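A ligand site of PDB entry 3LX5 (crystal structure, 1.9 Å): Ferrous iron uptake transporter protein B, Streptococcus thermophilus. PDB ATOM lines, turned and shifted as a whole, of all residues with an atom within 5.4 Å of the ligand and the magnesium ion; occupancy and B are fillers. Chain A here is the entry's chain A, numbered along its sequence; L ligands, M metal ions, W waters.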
ATOM      1  N   GLY A  10       0.306 -16.562  25.705  1.00  0.00           N
ATOM      2  CA  GLY A  10       0.201 -17.239  24.412  1.00  0.00           C
ATOM      3  C   GLY A  10       1.522 -17.832  24.013  1.00  0.00           C
ATOM      4  O   GLY A  10       2.553 -17.524  24.620  1.00  0.00           O
ATOM      5  N   ASN A  11       1.506 -18.663  22.979  1.00  0.00           N
ATOM      6  CA  ASN A  11       2.763 -19.279  22.514  1.00  0.00           C
ATOM      7  C   ASN A  11       3.760 -18.186  22.089  1.00  0.00           C
ATOM      8  O   ASN A  11       3.357 -17.085  21.690  1.00  0.00           O
ATOM      9  CB  ASN A  11       2.549 -20.237  21.322  1.00  0.00           C
ATOM     10  CG  ASN A  11       1.586 -21.383  21.612  1.00  0.00           C
ATOM     11  OD1 ASN A  11       1.188 -22.054  20.668  1.00  0.00           O
ATOM     12  ND2 ASN A  11       1.225 -21.624  22.882  1.00  0.00           N
ATOM     13  N   PRO A  12       5.069 -18.472  22.193  1.00  0.00           N
ATOM     14  CA  PRO A  12       6.009 -17.514  21.612  1.00  0.00           C
ATOM     15  C   PRO A  12       5.755 -17.338  20.101  1.00  0.00           C
ATOM     16  O   PRO A  12       5.284 -18.267  19.443  1.00  0.00           O
ATOM     17  CB  PRO A  12       7.391 -18.146  21.827  1.00  0.00           C
ATOM     18  CG  PRO A  12       7.193 -19.301  22.789  1.00  0.00           C
ATOM     19  CD  PRO A  12       5.736 -19.663  22.762  1.00  0.00           C
ATOM     20  N   ASN A  13       6.077 -16.145  19.602  1.00  0.00           N
ATOM     21  CA  ASN A  13       6.038 -15.798  18.174  1.00  0.00           C
ATOM     22  C   ASN A  13       4.564 -15.770  17.713  1.00  0.00           C
ATOM     23  O   ASN A  13       4.281 -16.165  16.581  1.00  0.00           O
ATOM     24  CB  ASN A  13       6.894 -16.815  17.378  1.00  0.00           C
ATOM     25  CG  ASN A  13       7.339 -16.335  15.982  1.00  0.00           C
ATOM     26  OD1 ASN A  13       7.287 -15.142  15.641  1.00  0.00           O
ATOM     27  ND2 ASN A  13       7.818 -17.291  15.179  1.00  0.00           N
ATOM     28  N   SER A  14       3.646 -15.325  18.578  1.00  0.00           N
ATOM     29  CA  SER A  14       2.211 -15.247  18.234  1.00  0.00           C
ATOM     30  C   SER A  14       1.703 -13.799  18.045  1.00  0.00           C
ATOM     31  O   SER A  14       0.566 -13.583  17.595  1.00  0.00           O
ATOM     32  CB  SER A  14       1.351 -16.011  19.260  1.00  0.00           C
ATOM     33  OG  SER A  14       1.508 -15.517  20.597  1.00  0.00           O
ATOM     34  N   GLY A  15       2.583 -12.843  18.354  1.00  0.00           N
ATOM     35  CA  GLY A  15       2.323 -11.405  18.236  1.00  0.00           C
ATOM     36  C   GLY A  15       1.966 -10.725  19.555  1.00  0.00           C
ATOM     37  O   GLY A  15       1.334  -9.674  19.517  1.00  0.00           O
ATOM     38  N   LYS A  16       2.306 -11.302  20.716  1.00  0.00           N
ATOM     39  CA  LYS A  16       2.007 -10.639  21.995  1.00  0.00           C
ATOM     40  C   LYS A  16       2.587  -9.228  22.133  1.00  0.00           C
ATOM     41  O   LYS A  16       1.862  -8.259  22.395  1.00  0.00           O
ATOM     42  CB  LYS A  16       2.349 -11.502  23.233  1.00  0.00           C
ATOM     43  CG  LYS A  16       1.600 -12.867  23.246  1.00  0.00           C
ATOM     44  CD  LYS A  16       1.969 -13.700  24.515  1.00  0.00           C
ATOM     45  CE  LYS A  16       3.483 -13.988  24.542  1.00  0.00           C
ATOM     46  NZ  LYS A  16       3.993 -14.723  23.329  1.00  0.00           N
ATOM     47  N   THR A  17       3.893  -9.092  21.969  1.00  0.00           N
ATOM     48  CA  THR A  17       4.512  -7.778  22.081  1.00  0.00           C
ATOM     49  C   THR A  17       4.024  -6.824  20.991  1.00  0.00           C
ATOM     50  O   THR A  17       3.816  -5.646  21.257  1.00  0.00           O
ATOM     51  CB  THR A  17       6.037  -7.890  22.120  1.00  0.00           C
ATOM     52  OG1 THR A  17       6.387  -8.839  23.127  1.00  0.00           O
ATOM     53  CG2 THR A  17       6.662  -6.563  22.517  1.00  0.00           C
ATOM     54  N   SER A  18       3.810  -7.354  19.787  1.00  0.00           N
ATOM     55  CA  SER A  18       3.302  -6.500  18.702  1.00  0.00           C
ATOM     56  C   SER A  18       1.982  -5.870  19.148  1.00  0.00           C
ATOM     57  O   SER A  18       1.794  -4.666  18.982  1.00  0.00           O
ATOM     58  CB  SER A  18       3.129  -7.300  17.376  1.00  0.00           C
ATOM     59  OG  SER A  18       4.330  -7.933  16.961  1.00  0.00           O
ATOM     60  N   LEU A  19       1.071  -6.677  19.708  1.00  0.00           N
ATOM     61  CA  LEU A  19      -0.182  -6.119  20.216  1.00  0.00           C
ATOM     62  C   LEU A  19       0.035  -5.194  21.405  1.00  0.00           C
ATOM     63  O   LEU A  19      -0.548  -4.105  21.456  1.00  0.00           O
ATOM     64  CB  LEU A  19      -1.220  -7.211  20.563  1.00  0.00           C
ATOM     65  CG  LEU A  19      -1.586  -8.185  19.429  1.00  0.00           C
ATOM     66  CD1 LEU A  19      -2.167  -9.502  20.077  1.00  0.00           C
ATOM     67  CD2 LEU A  19      -2.589  -7.641  18.422  1.00  0.00           C
ATOM     68  N   ARG A  29      10.585  -4.982  22.327  1.00  0.00           N
ATOM     69  CA  ARG A  29      11.236  -5.842  21.332  1.00  0.00           C
ATOM     70  C   ARG A  29      10.278  -6.832  20.679  1.00  0.00           C
ATOM     71  O   ARG A  29       9.614  -7.643  21.361  1.00  0.00           O
ATOM     72  CB  ARG A  29      12.402  -6.589  21.987  1.00  0.00           C
ATOM     73  CG  ARG A  29      13.571  -5.701  22.254  1.00  0.00           C
ATOM     74  CD  ARG A  29      14.775  -6.496  22.711  1.00  0.00           C
ATOM     75  NE  ARG A  29      15.861  -5.539  22.810  1.00  0.00           N
ATOM     76  CZ  ARG A  29      17.112  -5.818  23.157  1.00  0.00           C
ATOM     77  NH1 ARG A  29      17.476  -7.055  23.458  1.00  0.00           N
ATOM     78  NH2 ARG A  29      17.997  -4.849  23.212  1.00  0.00           N
ATOM     79  N   VAL A  30      10.225  -6.757  19.351  1.00  0.00           N
ATOM     80  CA  VAL A  30       9.416  -7.652  18.498  1.00  0.00           C
ATOM     81  C   VAL A  30      10.367  -8.297  17.476  1.00  0.00           C
ATOM     82  O   VAL A  30      11.193  -7.595  16.878  1.00  0.00           O
ATOM     83  CB  VAL A  30       8.312  -6.844  17.763  1.00  0.00           C
ATOM     84  CG1 VAL A  30       7.600  -7.693  16.621  1.00  0.00           C
ATOM     85  CG2 VAL A  30       7.305  -6.254  18.787  1.00  0.00           C
ATOM     86  N   GLY A  31      10.269  -9.606  17.267  1.00  0.00           N
ATOM     87  CA  GLY A  31      11.161 -10.279  16.307  1.00  0.00           C
ATOM     88  C   GLY A  31      10.485 -11.504  15.722  1.00  0.00           C
ATOM     89  O   GLY A  31       9.525 -12.008  16.309  1.00  0.00           O
ATOM     90  N   ASN A  32      10.993 -11.979  14.586  1.00  0.00           N
ATOM     91  CA  ASN A  32      10.380 -13.084  13.842  1.00  0.00           C
ATOM     92  C   ASN A  32      10.828 -14.473  14.303  1.00  0.00           C
ATOM     93  O   ASN A  32      10.950 -15.375  13.485  1.00  0.00           O
ATOM     94  CB  ASN A  32      10.650 -12.915  12.346  1.00  0.00           C
ATOM     95  CG  ASN A  32      12.135 -13.069  11.983  1.00  0.00           C
ATOM     96  OD1 ASN A  32      12.992 -13.003  12.853  1.00  0.00           O
ATOM     97  ND2 ASN A  32      12.443 -13.298  10.700  1.00  0.00           N
ATOM     98  N   TRP A  33      11.107 -14.647  15.594  1.00  0.00           N
ATOM     99  CA  TRP A  33      11.506 -15.952  16.128  1.00  0.00           C
ATOM    100  C   TRP A  33      10.945 -16.124  17.531  1.00  0.00           C
ATOM    101  O   TRP A  33      10.680 -15.137  18.218  1.00  0.00           O
ATOM    102  CB  TRP A  33      13.043 -16.146  16.101  1.00  0.00           C
ATOM    103  CG  TRP A  33      13.780 -15.362  17.157  1.00  0.00           C
ATOM    104  CD1 TRP A  33      14.125 -15.770  18.421  1.00  0.00           C
ATOM    105  CD2 TRP A  33      14.253 -14.014  17.027  1.00  0.00           C
ATOM    106  NE1 TRP A  33      14.790 -14.761  19.083  1.00  0.00           N
ATOM    107  CE2 TRP A  33      14.891 -13.670  18.251  1.00  0.00           C
ATOM    108  CE3 TRP A  33      14.197 -13.062  16.006  1.00  0.00           C
ATOM    109  CZ2 TRP A  33      15.459 -12.413  18.479  1.00  0.00           C
ATOM    110  CZ3 TRP A  33      14.771 -11.806  16.227  1.00  0.00           C
ATOM    111  CH2 TRP A  33      15.396 -11.501  17.461  1.00  0.00           C
ATOM    112  N   PRO A  34      10.745 -17.385  17.963  1.00  0.00           N
ATOM    113  CA  PRO A  34      10.165 -17.597  19.290  1.00  0.00           C
ATOM    114  C   PRO A  34      11.216 -17.354  20.374  1.00  0.00           C
ATOM    115  O   PRO A  34      12.350 -17.823  20.255  1.00  0.00           O
ATOM    116  CB  PRO A  34       9.707 -19.083  19.249  1.00  0.00           C
ATOM    117  CG  PRO A  34      10.523 -19.737  18.165  1.00  0.00           C
ATOM    118  CD  PRO A  34      10.938 -18.627  17.200  1.00  0.00           C
ATOM    119  N   GLY A  35      10.836 -16.607  21.415  1.00  0.00           N
ATOM    120  CA  GLY A  35      11.702 -16.369  22.566  1.00  0.00           C
ATOM    121  C   GLY A  35      12.286 -14.972  22.617  1.00  0.00           C
ATOM    122  O   GLY A  35      13.397 -14.777  23.103  1.00  0.00           O
ATOM    123  N   VAL A  36      11.547 -13.997  22.112  1.00  0.00           N
ATOM    124  CA  VAL A  36      12.039 -12.611  22.071  1.00  0.00           C
ATOM    125  C   VAL A  36      11.903 -11.974  23.457  1.00  0.00           C
ATOM    126  O   VAL A  36      12.906 -11.545  24.014  1.00  0.00           O
ATOM    127  CB  VAL A  36      11.426 -11.786  20.899  1.00  0.00           C
ATOM    128  CG1 VAL A  36      11.755 -10.273  21.025  1.00  0.00           C
ATOM    129  CG2 VAL A  36      11.958 -12.321  19.528  1.00  0.00           C
ATOM    130  N   THR A  37      10.686 -11.968  24.019  1.00  0.00           N
ATOM    131  CA  THR A  37      10.428 -11.341  25.301  1.00  0.00           C
ATOM    132  C   THR A  37      10.893 -12.296  26.384  1.00  0.00           C
ATOM    133  O   THR A  37      10.598 -13.506  26.304  1.00  0.00           O
ATOM    134  CB  THR A  37       8.897 -11.065  25.451  1.00  0.00           C
ATOM    135  OG1 THR A  37       8.479 -10.209  24.349  1.00  0.00           O
ATOM    136  CG2 THR A  37       8.534 -10.450  26.805  1.00  0.00           C
ATOM    137  N   ASP A  55       2.849  -7.576  29.196  1.00  0.00           N
ATOM    138  CA  ASP A  55       3.527  -8.402  28.189  1.00  0.00           C
ATOM    139  C   ASP A  55       4.401  -9.438  28.934  1.00  0.00           C
ATOM    140  O   ASP A  55       5.106  -9.113  29.898  1.00  0.00           O
ATOM    141  CB  ASP A  55       4.359  -7.518  27.247  1.00  0.00           C
ATOM    142  CG  ASP A  55       4.858  -8.279  26.017  1.00  0.00           C
ATOM    143  OD1 ASP A  55       4.275  -9.354  25.723  1.00  0.00           O
ATOM    144  OD2 ASP A  55       5.857  -7.829  25.395  1.00  0.00           O
ATOM    145  N   LEU A  56       4.292 -10.703  28.531  1.00  0.00           N
ATOM    146  CA  LEU A  56       5.017 -11.803  29.158  1.00  0.00           C
ATOM    147  C   LEU A  56       5.720 -12.655  28.112  1.00  0.00           C
ATOM    148  O   LEU A  56       5.264 -12.667  26.962  1.00  0.00           O
ATOM    149  CB  LEU A  56       4.028 -12.681  29.962  1.00  0.00           C
ATOM    150  CG  LEU A  56       3.739 -11.986  31.323  1.00  0.00           C
ATOM    151  CD1 LEU A  56       2.476 -12.499  31.794  1.00  0.00           C
ATOM    152  CD2 LEU A  56       4.816 -12.240  32.374  1.00  0.00           C
ATOM    153  N   PRO A  57       6.819 -13.351  28.483  1.00  0.00           N
ATOM    154  CA  PRO A  57       7.422 -14.295  27.543  1.00  0.00           C
ATOM    155  C   PRO A  57       6.395 -15.344  27.085  1.00  0.00           C
ATOM    156  O   PRO A  57       5.496 -15.707  27.856  1.00  0.00           O
ATOM    157  CB  PRO A  57       8.541 -14.967  28.357  1.00  0.00           C
ATOM    158  CG  PRO A  57       8.872 -13.955  29.439  1.00  0.00           C
ATOM    159  CD  PRO A  57       7.516 -13.389  29.800  1.00  0.00           C
ATOM    160  N   GLY A  58       6.490 -15.798  25.825  1.00  0.00           N
ATOM    161  CA  GLY A  58       5.603 -16.873  25.346  1.00  0.00           C
ATOM    162  C   GLY A  58       5.764 -18.188  26.091  1.00  0.00           C
ATOM    163  O   GLY A  58       6.814 -18.482  26.669  1.00  0.00           O
ATOM    164  N   ASN A 115      -5.089 -13.880  16.560  1.00  0.00           N
ATOM    165  CA  ASN A 115      -4.145 -13.019  15.870  1.00  0.00           C
ATOM    166  C   ASN A 115      -3.560 -13.612  14.570  1.00  0.00           C
ATOM    167  O   ASN A 115      -3.767 -14.788  14.264  1.00  0.00           O
ATOM    168  CB  ASN A 115      -3.022 -12.623  16.861  1.00  0.00           C
ATOM    169  CG  ASN A 115      -2.256 -11.392  16.421  1.00  0.00           C
ATOM    170  OD1 ASN A 115      -2.833 -10.395  15.971  1.00  0.00           O
ATOM    171  ND2 ASN A 115      -0.936 -11.458  16.526  1.00  0.00           N
ATOM    172  N   MET A 116      -2.817 -12.781  13.831  1.00  0.00           N
ATOM    173  CA  MET A 116      -2.283 -13.150  12.506  1.00  0.00           C
ATOM    174  C   MET A 116      -3.418 -13.528  11.581  1.00  0.00           C
ATOM    175  O   MET A 116      -3.271 -14.367  10.692  1.00  0.00           O
ATOM    176  CB  MET A 116      -1.256 -14.266  12.634  1.00  0.00           C
ATOM    177  CG  MET A 116       0.000 -13.781  13.333  1.00  0.00           C
ATOM    178  SD  MET A 116       1.087 -15.101  13.908  1.00  0.00           S
ATOM    179  CE  MET A 116       2.407 -14.056  14.530  1.00  0.00           C
ATOM    180  N   ILE A 117      -4.577 -12.911  11.794  1.00  0.00           N
ATOM    181  CA  ILE A 117      -5.716 -13.209  10.942  1.00  0.00           C
ATOM    182  C   ILE A 117      -5.416 -12.831   9.481  1.00  0.00           C
ATOM    183  O   ILE A 117      -5.956 -13.443   8.561  1.00  0.00           O
ATOM    184  CB  ILE A 117      -7.039 -12.550  11.433  1.00  0.00           C
ATOM    185  CG1 ILE A 117      -8.265 -13.380  10.995  1.00  0.00           C
ATOM    186  CG2 ILE A 117      -7.144 -11.098  10.936  1.00  0.00           C
ATOM    187  CD1 ILE A 117      -8.340 -14.792  11.636  1.00  0.00           C
ATOM    188  N   ASP A 118      -4.537 -11.854   9.260  1.00  0.00           N
ATOM    189  CA  ASP A 118      -4.215 -11.428   7.890  1.00  0.00           C
ATOM    190  C   ASP A 118      -3.438 -12.506   7.131  1.00  0.00           C
ATOM    191  O   ASP A 118      -3.516 -12.603   5.913  1.00  0.00           O
ATOM    192  CB  ASP A 118      -3.372 -10.143   7.908  1.00  0.00           C
ATOM    193  CG  ASP A 118      -2.119 -10.290   8.753  1.00  0.00           C
ATOM    194  OD1 ASP A 118      -2.220 -10.473  10.009  1.00  0.00           O
ATOM    195  OD2 ASP A 118      -1.035 -10.245   8.158  1.00  0.00           O
ATOM    196  N   VAL A 119      -2.681 -13.319   7.874  1.00  0.00           N
ATOM    197  CA  VAL A 119      -1.877 -14.391   7.286  1.00  0.00           C
ATOM    198  C   VAL A 119      -2.803 -15.501   6.861  1.00  0.00           C
ATOM    199  O   VAL A 119      -2.674 -16.057   5.761  1.00  0.00           O
ATOM    200  CB  VAL A 119      -0.804 -14.947   8.277  1.00  0.00           C
ATOM    201  CG1 VAL A 119       0.081 -15.983   7.577  1.00  0.00           C
ATOM    202  CG2 VAL A 119       0.038 -13.820   8.826  1.00  0.00           C
ATOM    203  N   THR A 143      -7.827 -10.595  15.237  1.00  0.00           N
ATOM    204  CA  THR A 143      -6.940  -9.445  15.283  1.00  0.00           C
ATOM    205  C   THR A 143      -5.789  -9.588  14.289  1.00  0.00           C
ATOM    206  O   THR A 143      -5.374 -10.711  13.896  1.00  0.00           O
ATOM    207  CB  THR A 143      -6.318  -9.200  16.704  1.00  0.00           C
ATOM    208  OG1 THR A 143      -5.482 -10.304  17.079  1.00  0.00           O
ATOM    209  CG2 THR A 143      -7.401  -9.024  17.764  1.00  0.00           C
ATOM    210  N   SER A 144      -5.289  -8.454  13.851  1.00  0.00           N
ATOM    211  CA  SER A 144      -4.017  -8.415  13.165  1.00  0.00           C
ATOM    212  C   SER A 144      -3.221  -7.251  13.733  1.00  0.00           C
ATOM    213  O   SER A 144      -3.615  -6.103  13.573  1.00  0.00           O
ATOM    214  CB  SER A 144      -4.201  -8.232  11.659  1.00  0.00           C
ATOM    215  OG  SER A 144      -2.945  -8.097  11.033  1.00  0.00           O
ATOM    216  N   ALA A 145      -2.096  -7.557  14.379  1.00  0.00           N
ATOM    217  CA  ALA A 145      -1.141  -6.507  14.761  1.00  0.00           C
ATOM    218  C   ALA A 145      -0.466  -5.892  13.539  1.00  0.00           C
ATOM    219  O   ALA A 145       0.026  -4.765  13.633  1.00  0.00           O
ATOM    220  CB  ALA A 145      -0.105  -7.019  15.765  1.00  0.00           C
ATOM    221  N   LEU A 146      -0.444  -6.598  12.403  1.00  0.00           N
ATOM    222  CA  LEU A 146       0.162  -6.036  11.212  1.00  0.00           C
ATOM    223  C   LEU A 146      -0.756  -4.995  10.575  1.00  0.00           C
ATOM    224  O   LEU A 146      -0.360  -3.841  10.419  1.00  0.00           O
ATOM    225  CB  LEU A 146       0.576  -7.095  10.172  1.00  0.00           C
ATOM    226  CG  LEU A 146       1.275  -6.539   8.928  1.00  0.00           C
ATOM    227  CD1 LEU A 146       2.678  -5.952   9.236  1.00  0.00           C
ATOM    228  CD2 LEU A 146       1.333  -7.589   7.790  1.00  0.00           C
HETATM  229  O1  LIG L   1       7.776 -10.681  13.297  1.00  0.00           O
HETATM  230  C1  LIG L   1       6.960 -10.541  14.518  1.00  0.00           C
HETATM  231  C2  LIG L   1       5.815  -9.801  13.869  1.00  0.00           C
HETATM  232  O2  LIG L   1       5.898  -8.717  13.278  1.00  0.00           O
HETATM  233  C3  LIG L   1       6.418 -11.929  14.866  1.00  0.00           C
HETATM  234  C4  LIG L   1       6.316 -12.180  16.378  1.00  0.00           C
HETATM  235  O3  LIG L   1       5.787 -10.978  17.030  1.00  0.00           O
HETATM  236  P1  LIG L   1       6.088 -10.745  18.549  1.00  0.00           P
HETATM  237  O4  LIG L   1       5.161  -9.657  18.878  1.00  0.00           O
HETATM  238  O5  LIG L   1       7.531 -10.638  18.834  1.00  0.00           O
HETATM  239  O6  LIG L   1       5.599 -12.224  19.206  1.00  0.00           O
HETATM  240  P2  LIG L   1       5.582 -12.650  20.775  1.00  0.00           P
HETATM  241  O7  LIG L   1       4.325 -13.409  20.915  1.00  0.00           O
HETATM  242  O8  LIG L   1       5.740 -11.425  21.621  1.00  0.00           O
HETATM  243  N1  LIG L   1       6.854 -13.656  20.853  1.00  0.00           N
HETATM  244  P3  LIG L   1       7.544 -13.888  22.327  1.00  0.00           P
HETATM  245  O9  LIG L   1       6.410 -14.697  23.177  1.00  0.00           O
HETATM  246  O10 LIG L   1       8.812 -14.826  22.049  1.00  0.00           O
HETATM  247  O11 LIG L   1       8.047 -12.600  22.909  1.00  0.00           O
HETATM  248  O12 LIG L   1       5.071 -12.030  14.395  1.00  0.00           O
HETATM  249  C5  LIG L   1       4.709 -10.832  13.620  1.00  0.00           C
HETATM  250  N2  LIG L   1       3.312 -10.543  13.910  1.00  0.00           N
HETATM  251  C6  LIG L   1       2.745 -10.308  15.100  1.00  0.00           C
HETATM  252  N3  LIG L   1       1.434 -10.140  14.899  1.00  0.00           N
HETATM  253  C7  LIG L   1       1.164 -10.277  13.589  1.00  0.00           C
HETATM  254  C8  LIG L   1       2.364 -10.536  12.958  1.00  0.00           C
HETATM  255  N4  LIG L   1       2.417 -10.733  11.620  1.00  0.00           N
HETATM  256  C9  LIG L   1       1.317 -10.660  10.870  1.00  0.00           C
HETATM  257  N5  LIG L   1       1.427 -10.847   9.553  1.00  0.00           N
HETATM  258  N6  LIG L   1       0.055 -10.393  11.432  1.00  0.00           N
HETATM  259  C10 LIG L   1      -0.007 -10.209  12.819  1.00  0.00           C
HETATM  260  O13 LIG L   1      -1.089  -9.979  13.330  1.00  0.00           O
HETATM  261 MG    MG M   1       7.035 -10.861  22.996  1.00  0.00          MG
HETATM  262  O   HOH W   1       8.700 -13.340  18.739  1.00  0.00           O
HETATM  263  O   HOH W   2       8.325 -10.049  21.233  1.00  0.00           O
HETATM  264  O   HOH W   3       9.538 -15.388  24.797  1.00  0.00           O
HETATM  265  O   HOH W   4       5.760 -11.340  24.582  1.00  0.00           O
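The backbone NH of Ala 145 sits at hydrogen-bond distance from an oxygen (O13) of the ligand (2.8 Å). An oxygen (O13) of the ligand is in hydrogen-bond range of the backbone NH of Met 116, at 3.3 Å. The backbone NH of Lys 16 lies within hydrogen-bond range of an oxygen (O7) of the ligand. An oxygen (O10) of the ligand lies within hydrogen-bond range of the backbone NH (N) of Val 36 (2.9 Å). The backbone NH of Gly 31 sits at hydrogen-bond distance from an oxygen (O5) of the ligand. N of Ser 14 sits at hydrogen-bond distance from O7 of the ligand, at 3.1 Å. O7 of the ligand is in hydrogen-bond range of N of Gly 15 (3.1 Å). An oxygen (O9) of the ligand lies within hydrogen-bond range of the backbone NH (N) of Gly 58, 2.9 Å away. N3 of the ligand is in hydrogen-bond range of ND2 of Asn 115. O10 of the ligand is in hydrogen-bond range of N of Gly 35, 2.8 Å away. An oxygen (O4) of the ligand is in hydrogen-bond range of the side-chain hydroxyl (OG) of Ser 18, at 2.7 Å. N of Thr 37 lies close to O11 of the ligand (2.9 Å). The side-chain amino group (NZ) of Lys 16 lies within salt-bridge range of an oxygen (O9) of the ligand, at 2.4 Å. The backbone NH (N) of Ser 18 sits at hydrogen-bond distance from an oxygen (O4) of the ligand. The backbone NH (N) of Thr 17 lies within hydrogen-bond range of an oxygen (O4) of the ligand (3.4 Å). A nitrogen (N6) of the ligand is in hydrogen-bond range of the side-chain carboxylate of Asp 118, 2.7 Å away.
The backbone carbonyl oxygen (O) of Thr 143 sits at hydrogen-bond distance from the backbone NH (N) of Met 116 (3.3 Å). The side-chain hydroxyl (OG) of Ser 144 lies within hydrogen-bond range of the side-chain carboxylate (OD1) of Asp 118 (2.7 Å). The side-chain hydroxyl (OG) of Ser 14 lies within hydrogen-bond range of the backbone carbonyl oxygen (O) of Asn 11, at 2.7 Å. The side-chain amide oxygen (OD1) of Asn 115 sits at hydrogen-bond distance from the backbone NH (N) of Ala 145 (3.3 Å). The side-chain amide oxygen of Asn 115 sits at hydrogen-bond distance from the side-chain hydroxyl of Thr 143, at 2.9 Å. The side-chain amino group (NZ) of Lys 16 is in hydrogen-bond range of the backbone carbonyl oxygen (O) of Asn 11, 2.9 Å away. The backbone carbonyl oxygen (O) of Ser 14 is in hydrogen-bond range of the side-chain amide nitrogen (ND2) of Asn 115 (2.8 Å). OG of Ser 144 lies close to N of Leu 146.
The backbone NH (N) of Asn 13 lies close to a nitrogen (N1) of the ligand (2.9 Å). Merely in contact with the ligand: Asn 11 (3.9 Å), Pro 12 (3.2 Å), Val 30 (3.5 Å), Asn 32 (3.6 Å), Pro 34 (3.9 Å), Pro 57 (3.96 Å), Val 119 (3.4 Å), Ser 144 (3.3 Å) and Leu 146 (3.6 Å). Hydrophobic or aromatic side chains that line the ligand: Pro 12, Val 30, Met 116, Val 119, Ala 145 and Leu 146. Of the 32 residues printed, 24 come within 4 Å of the ligand.
Two residues have an atom within 4 Å of the magnesium ion: Thr 17 and Thr 37.
The magnesium ion is bound by an oxygen (O8) of the ligand (2.0 Å), an oxygen (O11) of the ligand (2.0 Å), the side-chain hydroxyl of Thr 37 (2.1 Å), water W4 (2.1 Å), the side-chain hydroxyl of Thr 17 (2.1 Å) and water W2 (2.3 Å).
Water W4 lies within hydrogen-bond range of the side-chain carboxylate of Asp 55 (2.7 Å) and the backbone carbonyl oxygen of Leu 56 (2.8 Å). Water W2 lies within hydrogen-bond range of an oxygen (O5) of the ligand and the backbone carbonyl oxygen (O) of Arg 29. Water W1 lies within hydrogen-bond range of the backbone carbonyl oxygen of Trp 33 (2.7 Å), a nitrogen (N1) of the ligand (2.8 Å) and the backbone carbonyl oxygen of Gly 31 (2.9 Å). Water W3 lies within hydrogen-bond range of O of Thr 37 (2.6 Å), O10 of the ligand (2.9 Å) and N of Gly 58 (3.2 Å).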
